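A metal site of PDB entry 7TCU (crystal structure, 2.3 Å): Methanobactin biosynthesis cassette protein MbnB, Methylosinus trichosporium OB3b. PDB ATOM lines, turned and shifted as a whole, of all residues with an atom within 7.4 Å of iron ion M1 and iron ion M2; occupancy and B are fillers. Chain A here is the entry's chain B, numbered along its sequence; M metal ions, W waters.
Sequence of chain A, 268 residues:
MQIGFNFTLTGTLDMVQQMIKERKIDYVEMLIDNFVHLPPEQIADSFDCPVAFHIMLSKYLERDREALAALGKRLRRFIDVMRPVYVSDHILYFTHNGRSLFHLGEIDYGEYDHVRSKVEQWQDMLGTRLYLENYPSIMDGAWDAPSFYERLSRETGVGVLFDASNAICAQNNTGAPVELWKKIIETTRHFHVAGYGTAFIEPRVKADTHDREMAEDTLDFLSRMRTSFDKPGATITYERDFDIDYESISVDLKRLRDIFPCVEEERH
Iron ion M2 is bound by the side-chain carboxylate of Asp 163, water W4, the side-chain carboxylate of Glu 133, a ring nitrogen (ND1) of His 192, the side-chain carboxylate of Glu 239 and water W3. Iron ion M2 has six donor atoms within binding distance.
The side-chain hydroxyl (OG) of Ser 165 sits at hydrogen-bond distance from the side-chain carboxylate (OD1) of Asp 163 (3.0 Å). The side-chain amide oxygen of Asn 134 lies within hydrogen-bond range of the backbone NH of Asp 163, 2.7 Å away. The side-chain sulfur (SD) of Met 56 lies close to a ring nitrogen (NE2) of His 90, 3.6 Å away. The backbone carbonyl oxygen (O) of Ile 55 lies within hydrogen-bond range of a ring nitrogen (ND1) of His 90, 2.8 Å away. The side-chain hydroxyl (OG) of Ser 88 sits at hydrogen-bond distance from a ring nitrogen (ND1) of His 54, 2.9 Å away. N of Glu 133 sits at hydrogen-bond distance from O of Asp 89 (3.1 Å). O of His 192 lies within hydrogen-bond range of N of Ala 164, at 2.9 Å. N of His 192 is in hydrogen-bond range of O of Phe 162 (2.9 Å).
Of the 26 residues printed, 3 come within 4 Å of iron ion M1. The nearest printed residue that does not touch iron ion M1 is His 192 (4.4 Å).
Iron ion M1 is bound by water W3 (1.8 Å), NE2 of His 90 (2.0 Å), water W2 (2.1 Å), NE2 of His 54 (2.1 Å), OE1 of Glu 133 (2.3 Å) and water W1 (2.4 Å). Iron ion M1 has six donor atoms within binding distance.
Within 4 Å of iron ion M2: Glu 133, Asp 163, His 192 and Glu 239. The nearest printed residue that does not touch iron ion M2 is His 210 (4.5 Å).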
ATOM      1  N   GLU A  29      21.382  15.336 -14.972  1.00  0.00           N
ATOM      2  CA  GLU A  29      21.192  15.968 -13.676  1.00  0.00           C
ATOM      3  C   GLU A  29      20.528  14.975 -12.713  1.00  0.00           C
ATOM      4  O   GLU A  29      19.339  14.677 -12.858  1.00  0.00           O
ATOM      5  CB  GLU A  29      20.358  17.236 -13.795  1.00  0.00           C
ATOM      6  CG  GLU A  29      20.231  17.953 -12.484  1.00  0.00           C
ATOM      7  CD  GLU A  29      19.503  19.266 -12.658  1.00  0.00           C
ATOM      8  OE1 GLU A  29      20.130  20.267 -13.071  1.00  0.00           O
ATOM      9  OE2 GLU A  29      18.293  19.281 -12.413  1.00  0.00           O
ATOM     10  N   LEU A  31      18.730  13.827  -9.445  1.00  0.00           N
ATOM     11  CA  LEU A  31      18.022  14.209  -8.218  1.00  0.00           C
ATOM     12  C   LEU A  31      18.661  13.405  -7.089  1.00  0.00           C
ATOM     13  O   LEU A  31      18.180  12.342  -6.672  1.00  0.00           O
ATOM     14  CB  LEU A  31      16.520  13.988  -8.362  1.00  0.00           C
ATOM     15  CG  LEU A  31      15.634  14.612  -7.253  1.00  0.00           C
ATOM     16  CD1 LEU A  31      15.817  16.121  -7.206  1.00  0.00           C
ATOM     17  CD2 LEU A  31      14.155  14.306  -7.500  1.00  0.00           C
ATOM     18  N   HIS A  54      20.997  17.843  -8.293  1.00  0.00           N
ATOM     19  CA  HIS A  54      19.858  18.646  -7.869  1.00  0.00           C
ATOM     20  C   HIS A  54      19.365  18.038  -6.566  1.00  0.00           C
ATOM     21  O   HIS A  54      19.083  16.832  -6.517  1.00  0.00           O
ATOM     22  CB  HIS A  54      18.785  18.631  -8.961  1.00  0.00           C
ATOM     23  CG  HIS A  54      17.792  19.738  -8.852  1.00  0.00           C
ATOM     24  ND1 HIS A  54      18.130  21.027  -8.505  1.00  0.00           N
ATOM     25  CD2 HIS A  54      16.449  19.747  -9.062  1.00  0.00           C
ATOM     26  CE1 HIS A  54      17.051  21.781  -8.501  1.00  0.00           C
ATOM     27  NE2 HIS A  54      16.017  21.030  -8.835  1.00  0.00           N
ATOM     28  N   ILE A  55      19.326  18.820  -5.490  1.00  0.00           N
ATOM     29  CA  ILE A  55      18.910  18.330  -4.171  1.00  0.00           C
ATOM     30  C   ILE A  55      17.503  18.835  -3.897  1.00  0.00           C
ATOM     31  O   ILE A  55      17.241  20.048  -3.946  1.00  0.00           O
ATOM     32  CB  ILE A  55      19.880  18.782  -3.057  1.00  0.00           C
ATOM     33  CG1 ILE A  55      21.300  18.312  -3.350  1.00  0.00           C
ATOM     34  CG2 ILE A  55      19.425  18.314  -1.679  1.00  0.00           C
ATOM     35  CD1 ILE A  55      22.331  19.208  -2.690  1.00  0.00           C
ATOM     36  N   MET A  56      16.580  17.907  -3.602  1.00  0.00           N
ATOM     37  CA  MET A  56      15.179  18.250  -3.393  1.00  0.00           C
ATOM     38  C   MET A  56      14.823  18.413  -1.919  1.00  0.00           C
ATOM     39  O   MET A  56      14.236  19.425  -1.537  1.00  0.00           O
ATOM     40  CB  MET A  56      14.275  17.187  -4.044  1.00  0.00           C
ATOM     41  CG  MET A  56      12.821  17.604  -4.335  1.00  0.00           C
ATOM     42  SD  MET A  56      12.571  19.343  -4.837  1.00  0.00           S
ATOM     43  CE  MET A  56      11.060  19.780  -3.988  1.00  0.00           C
ATOM     44  N   SER A  88      22.970  21.819  -6.784  1.00  0.00           N
ATOM     45  CA  SER A  88      21.883  22.783  -6.662  1.00  0.00           C
ATOM     46  C   SER A  88      20.809  22.287  -5.708  1.00  0.00           C
ATOM     47  O   SER A  88      20.670  21.085  -5.443  1.00  0.00           O
ATOM     48  CB  SER A  88      21.262  23.106  -8.017  1.00  0.00           C
ATOM     49  OG  SER A  88      20.867  21.904  -8.643  1.00  0.00           O
ATOM     50  N   ASP A  89      20.050  23.258  -5.184  1.00  0.00           N
ATOM     51  CA  ASP A  89      18.996  23.052  -4.209  1.00  0.00           C
ATOM     52  C   ASP A  89      17.916  24.109  -4.455  1.00  0.00           C
ATOM     53  O   ASP A  89      17.894  24.775  -5.485  1.00  0.00           O
ATOM     54  CB  ASP A  89      19.577  23.097  -2.794  1.00  0.00           C
ATOM     55  CG  ASP A  89      18.706  22.345  -1.751  1.00  0.00           C
ATOM     56  OD1 ASP A  89      17.465  22.553  -1.720  1.00  0.00           O
ATOM     57  OD2 ASP A  89      19.286  21.598  -0.933  1.00  0.00           O
ATOM     58  N   HIS A  90      17.014  24.252  -3.493  1.00  0.00           N
ATOM     59  CA  HIS A  90      15.815  25.036  -3.672  1.00  0.00           C
ATOM     60  C   HIS A  90      15.658  26.027  -2.523  1.00  0.00           C
ATOM     61  O   HIS A  90      16.309  25.923  -1.491  1.00  0.00           O
ATOM     62  CB  HIS A  90      14.570  24.151  -3.709  1.00  0.00           C
ATOM     63  CG  HIS A  90      14.586  23.140  -4.803  1.00  0.00           C
ATOM     64  ND1 HIS A  90      15.353  22.001  -4.733  1.00  0.00           N
ATOM     65  CD2 HIS A  90      13.941  23.106  -5.991  1.00  0.00           C
ATOM     66  CE1 HIS A  90      15.190  21.311  -5.843  1.00  0.00           C
ATOM     67  NE2 HIS A  90      14.315  21.943  -6.616  1.00  0.00           N
ATOM     68  N   LEU A  92      12.396  26.782  -0.579  1.00  0.00           N
ATOM     69  CA  LEU A  92      11.068  26.225  -0.527  1.00  0.00           C
ATOM     70  C   LEU A  92      10.593  26.180   0.915  1.00  0.00           C
ATOM     71  O   LEU A  92      11.390  25.987   1.840  1.00  0.00           O
ATOM     72  CB  LEU A  92      11.063  24.818  -1.136  1.00  0.00           C
ATOM     73  CG  LEU A  92      11.040  24.668  -2.653  1.00  0.00           C
ATOM     74  CD1 LEU A  92      11.192  23.186  -2.988  1.00  0.00           C
ATOM     75  CD2 LEU A  92       9.707  25.188  -3.177  1.00  0.00           C
ATOM     76  N   GLU A 133      17.387  27.426  -7.007  1.00  0.00           N
ATOM     77  CA  GLU A 133      16.349  27.519  -8.024  1.00  0.00           C
ATOM     78  C   GLU A 133      15.260  28.538  -7.651  1.00  0.00           C
ATOM     79  O   GLU A 133      14.870  28.681  -6.479  1.00  0.00           O
ATOM     80  CB  GLU A 133      15.738  26.139  -8.244  1.00  0.00           C
ATOM     81  CG  GLU A 133      14.748  26.031  -9.386  1.00  0.00           C
ATOM     82  CD  GLU A 133      14.273  24.587  -9.593  1.00  0.00           C
ATOM     83  OE1 GLU A 133      14.759  23.680  -8.894  1.00  0.00           O
ATOM     84  OE2 GLU A 133      13.408  24.355 -10.444  1.00  0.00           O
ATOM     85  N   ASN A 134      14.727  29.198  -8.670  1.00  0.00           N
ATOM     86  CA  ASN A 134      13.623  30.125  -8.450  1.00  0.00           C
ATOM     87  C   ASN A 134      12.304  29.375  -8.365  1.00  0.00           C
ATOM     88  O   ASN A 134      12.102  28.326  -8.989  1.00  0.00           O
ATOM     89  CB  ASN A 134      13.556  31.172  -9.559  1.00  0.00           C
ATOM     90  CG  ASN A 134      13.643  30.561 -10.938  1.00  0.00           C
ATOM     91  OD1 ASN A 134      14.592  29.807 -11.228  1.00  0.00           O
ATOM     92  ND2 ASN A 134      12.673  30.891 -11.825  1.00  0.00           N
ATOM     93  N   LEU A 161      20.279  28.739 -10.127  1.00  0.00           N
ATOM     94  CA  LEU A 161      19.850  27.774 -11.117  1.00  0.00           C
ATOM     95  C   LEU A 161      18.542  28.331 -11.679  1.00  0.00           C
ATOM     96  O   LEU A 161      17.450  28.107 -11.147  1.00  0.00           O
ATOM     97  CB  LEU A 161      19.689  26.406 -10.488  1.00  0.00           C
ATOM     98  CG  LEU A 161      19.088  25.320 -11.379  1.00  0.00           C
ATOM     99  CD1 LEU A 161      19.929  25.182 -12.623  1.00  0.00           C
ATOM    100  CD2 LEU A 161      19.035  23.991 -10.614  1.00  0.00           C
ATOM    101  N   PHE A 162      18.640  29.115 -12.750  1.00  0.00           N
ATOM    102  CA  PHE A 162      17.466  29.801 -13.262  1.00  0.00           C
ATOM    103  C   PHE A 162      16.571  28.813 -14.000  1.00  0.00           C
ATOM    104  O   PHE A 162      16.984  28.231 -15.015  1.00  0.00           O
ATOM    105  CB  PHE A 162      17.840  30.946 -14.181  1.00  0.00           C
ATOM    106  CG  PHE A 162      16.654  31.650 -14.733  1.00  0.00           C
ATOM    107  CD1 PHE A 162      15.843  32.409 -13.887  1.00  0.00           C
ATOM    108  CD2 PHE A 162      16.311  31.520 -16.052  1.00  0.00           C
ATOM    109  CE1 PHE A 162      14.700  33.039 -14.369  1.00  0.00           C
ATOM    110  CE2 PHE A 162      15.172  32.182 -16.553  1.00  0.00           C
ATOM    111  CZ  PHE A 162      14.375  32.923 -15.697  1.00  0.00           C
ATOM    112  N   ASP A 163      15.356  28.647 -13.501  1.00  0.00           N
ATOM    113  CA  ASP A 163      14.376  27.740 -14.099  1.00  0.00           C
ATOM    114  C   ASP A 163      13.404  28.558 -14.929  1.00  0.00           C
ATOM    115  O   ASP A 163      12.580  29.301 -14.395  1.00  0.00           O
ATOM    116  CB  ASP A 163      13.641  26.964 -13.011  1.00  0.00           C
ATOM    117  CG  ASP A 163      12.771  25.824 -13.583  1.00  0.00           C
ATOM    118  OD1 ASP A 163      12.042  26.054 -14.594  1.00  0.00           O
ATOM    119  OD2 ASP A 163      12.819  24.696 -13.039  1.00  0.00           O
ATOM    120  N   ALA A 164      13.477  28.393 -16.244  1.00  0.00           N
ATOM    121  CA  ALA A 164      12.872  29.372 -17.135  1.00  0.00           C
ATOM    122  C   ALA A 164      11.349  29.185 -17.209  1.00  0.00           C
ATOM    123  O   ALA A 164      10.608  30.173 -17.154  1.00  0.00           O
ATOM    124  CB  ALA A 164      13.528  29.269 -18.515  1.00  0.00           C
ATOM    125  N   SER A 165      10.878  27.932 -17.259  1.00  0.00           N
ATOM    126  CA  SER A 165       9.437  27.668 -17.192  1.00  0.00           C
ATOM    127  C   SER A 165       8.829  28.088 -15.859  1.00  0.00           C
ATOM    128  O   SER A 165       7.676  28.509 -15.828  1.00  0.00           O
ATOM    129  CB  SER A 165       9.188  26.181 -17.452  1.00  0.00           C
ATOM    130  OG  SER A 165      10.170  25.359 -16.801  1.00  0.00           O
ATOM    131  N   ASN A 166       9.561  27.969 -14.754  1.00  0.00           N
ATOM    132  CA  ASN A 166       9.109  28.536 -13.480  1.00  0.00           C
ATOM    133  C   ASN A 166       8.928  30.054 -13.566  1.00  0.00           C
ATOM    134  O   ASN A 166       7.997  30.609 -12.972  1.00  0.00           O
ATOM    135  CB  ASN A 166      10.090  28.203 -12.363  1.00  0.00           C
ATOM    136  CG  ASN A 166       9.999  26.742 -11.935  1.00  0.00           C
ATOM    137  OD1 ASN A 166       9.267  25.969 -12.539  1.00  0.00           O
ATOM    138  ND2 ASN A 166      10.724  26.377 -10.889  1.00  0.00           N
ATOM    139  N   PHE A 191      20.696  26.426 -16.157  1.00  0.00           N
ATOM    140  CA  PHE A 191      19.277  26.653 -16.343  1.00  0.00           C
ATOM    141  C   PHE A 191      18.481  25.359 -16.287  1.00  0.00           C
ATOM    142  O   PHE A 191      19.016  24.259 -16.443  1.00  0.00           O
ATOM    143  CB  PHE A 191      19.019  27.338 -17.682  1.00  0.00           C
ATOM    144  CG  PHE A 191      19.771  28.615 -17.841  1.00  0.00           C
ATOM    145  CD1 PHE A 191      19.254  29.801 -17.330  1.00  0.00           C
ATOM    146  CD2 PHE A 191      21.003  28.636 -18.494  1.00  0.00           C
ATOM    147  CE1 PHE A 191      19.949  31.004 -17.463  1.00  0.00           C
ATOM    148  CE2 PHE A 191      21.692  29.817 -18.629  1.00  0.00           C
ATOM    149  CZ  PHE A 191      21.163  31.011 -18.108  1.00  0.00           C
ATOM    150  N   HIS A 192      17.180  25.519 -16.060  1.00  0.00           N
ATOM    151  CA  HIS A 192      16.187  24.462 -16.113  1.00  0.00           C
ATOM    152  C   HIS A 192      15.092  24.870 -17.102  1.00  0.00           C
ATOM    153  O   HIS A 192      14.829  26.067 -17.282  1.00  0.00           O
ATOM    154  CB  HIS A 192      15.550  24.232 -14.753  1.00  0.00           C
ATOM    155  CG  HIS A 192      16.240  23.200 -13.911  1.00  0.00           C
ATOM    156  ND1 HIS A 192      15.730  22.786 -12.702  1.00  0.00           N
ATOM    157  CD2 HIS A 192      17.384  22.516 -14.101  1.00  0.00           C
ATOM    158  CE1 HIS A 192      16.541  21.880 -12.181  1.00  0.00           C
ATOM    159  NE2 HIS A 192      17.555  21.706 -13.000  1.00  0.00           N
ATOM    160  N   VAL A 193      14.437  23.879 -17.711  1.00  0.00           N
ATOM    161  CA  VAL A 193      13.200  24.138 -18.460  1.00  0.00           C
ATOM    162  C   VAL A 193      12.376  22.862 -18.524  1.00  0.00           C
ATOM    163  O   VAL A 193      12.912  21.746 -18.431  1.00  0.00           O
ATOM    164  CB  VAL A 193      13.493  24.747 -19.870  1.00  0.00           C
ATOM    165  CG1 VAL A 193      14.065  23.737 -20.834  1.00  0.00           C
ATOM    166  CG2 VAL A 193      12.238  25.397 -20.446  1.00  0.00           C
ATOM    167  N   ALA A 194      11.060  23.018 -18.648  1.00  0.00           N
ATOM    168  CA  ALA A 194      10.106  21.935 -18.541  1.00  0.00           C
ATOM    169  C   ALA A 194       8.769  22.423 -19.065  1.00  0.00           C
ATOM    170  O   ALA A 194       8.560  23.611 -19.264  1.00  0.00           O
ATOM    171  CB  ALA A 194       9.948  21.455 -17.101  1.00  0.00           C
ATOM    172  N   ASP A 208       3.691  23.911 -11.988  1.00  0.00           N
ATOM    173  CA  ASP A 208       4.974  23.355 -12.449  1.00  0.00           C
ATOM    174  C   ASP A 208       4.939  21.814 -12.442  1.00  0.00           C
ATOM    175  O   ASP A 208       5.481  21.139 -11.573  1.00  0.00           O
ATOM    176  CB  ASP A 208       6.124  23.882 -11.597  1.00  0.00           C
ATOM    177  CG  ASP A 208       6.109  23.351 -10.153  1.00  0.00           C
ATOM    178  OD1 ASP A 208       5.098  23.529  -9.425  1.00  0.00           O
ATOM    179  OD2 ASP A 208       7.112  22.725  -9.756  1.00  0.00           O
ATOM    180  N   HIS A 210       5.983  19.500 -14.893  1.00  0.00           N
ATOM    181  CA  HIS A 210       7.036  18.728 -15.611  1.00  0.00           C
ATOM    182  C   HIS A 210       6.405  17.476 -16.197  1.00  0.00           C
ATOM    183  O   HIS A 210       6.951  16.389 -15.993  1.00  0.00           O
ATOM    184  CB  HIS A 210       8.235  18.426 -14.704  1.00  0.00           C
ATOM    185  CG  HIS A 210       8.608  19.524 -13.772  1.00  0.00           C
ATOM    186  ND1 HIS A 210       8.150  19.578 -12.476  1.00  0.00           N
ATOM    187  CD2 HIS A 210       9.412  20.597 -13.926  1.00  0.00           C
ATOM    188  CE1 HIS A 210       8.647  20.639 -11.881  1.00  0.00           C
ATOM    189  NE2 HIS A 210       9.422  21.274 -12.751  1.00  0.00           N
ATOM    190  N   THR A 237      18.987  22.022 -18.352  1.00  0.00           N
ATOM    191  CA  THR A 237      18.402  20.707 -18.098  1.00  0.00           C
ATOM    192  C   THR A 237      16.933  20.724 -18.473  1.00  0.00           C
ATOM    193  O   THR A 237      16.159  21.518 -17.925  1.00  0.00           O
ATOM    194  CB  THR A 237      18.495  20.341 -16.625  1.00  0.00           C
ATOM    195  OG1 THR A 237      19.834  20.540 -16.177  1.00  0.00           O
ATOM    196  CG2 THR A 237      18.044  18.892 -16.440  1.00  0.00           C
ATOM    197  N   GLU A 239      13.489  18.931 -17.913  1.00  0.00           N
ATOM    198  CA  GLU A 239      12.928  18.110 -16.840  1.00  0.00           C
ATOM    199  C   GLU A 239      11.602  17.505 -17.291  1.00  0.00           C
ATOM    200  O   GLU A 239      10.728  18.223 -17.791  1.00  0.00           O
ATOM    201  CB  GLU A 239      12.686  18.896 -15.571  1.00  0.00           C
ATOM    202  CG  GLU A 239      13.862  19.662 -15.061  1.00  0.00           C
ATOM    203  CD  GLU A 239      13.541  20.327 -13.739  1.00  0.00           C
ATOM    204  OE1 GLU A 239      12.818  21.340 -13.742  1.00  0.00           O
ATOM    205  OE2 GLU A 239      14.044  19.803 -12.696  1.00  0.00           O
ATOM    206  N   ASP A 241       9.107  14.833 -15.303  1.00  0.00           N
ATOM    207  CA  ASP A 241       8.887  14.020 -14.117  1.00  0.00           C
ATOM    208  C   ASP A 241       7.723  13.063 -14.253  1.00  0.00           C
ATOM    209  O   ASP A 241       7.605  12.138 -13.447  1.00  0.00           O
ATOM    210  CB  ASP A 241       8.628  14.895 -12.896  1.00  0.00           C
ATOM    211  CG  ASP A 241       9.745  15.849 -12.621  1.00  0.00           C
ATOM    212  OD1 ASP A 241      10.866  15.587 -13.118  1.00  0.00           O
ATOM    213  OD2 ASP A 241       9.515  16.846 -11.915  1.00  0.00           O
HETATM  214 FE    FE M   1      13.978  21.575  -8.574  1.00  0.00          FE
HETATM  215 FE    FE M   2      13.511  23.021 -12.208  1.00  0.00          FE
HETATM  216 FE    FE M   3       9.570  23.849 -13.480  1.00  0.00          FE
HETATM  217  O   HOH W   1      13.152  19.387  -8.188  1.00  0.00           O
HETATM  218  O   HOH W   2      12.001  22.301  -8.474  1.00  0.00           O
HETATM  219  O   HOH W   3      13.641  21.325 -10.367  1.00  0.00           O
HETATM  220  O   HOH W   4      11.484  22.963 -11.435  1.00  0.00           O
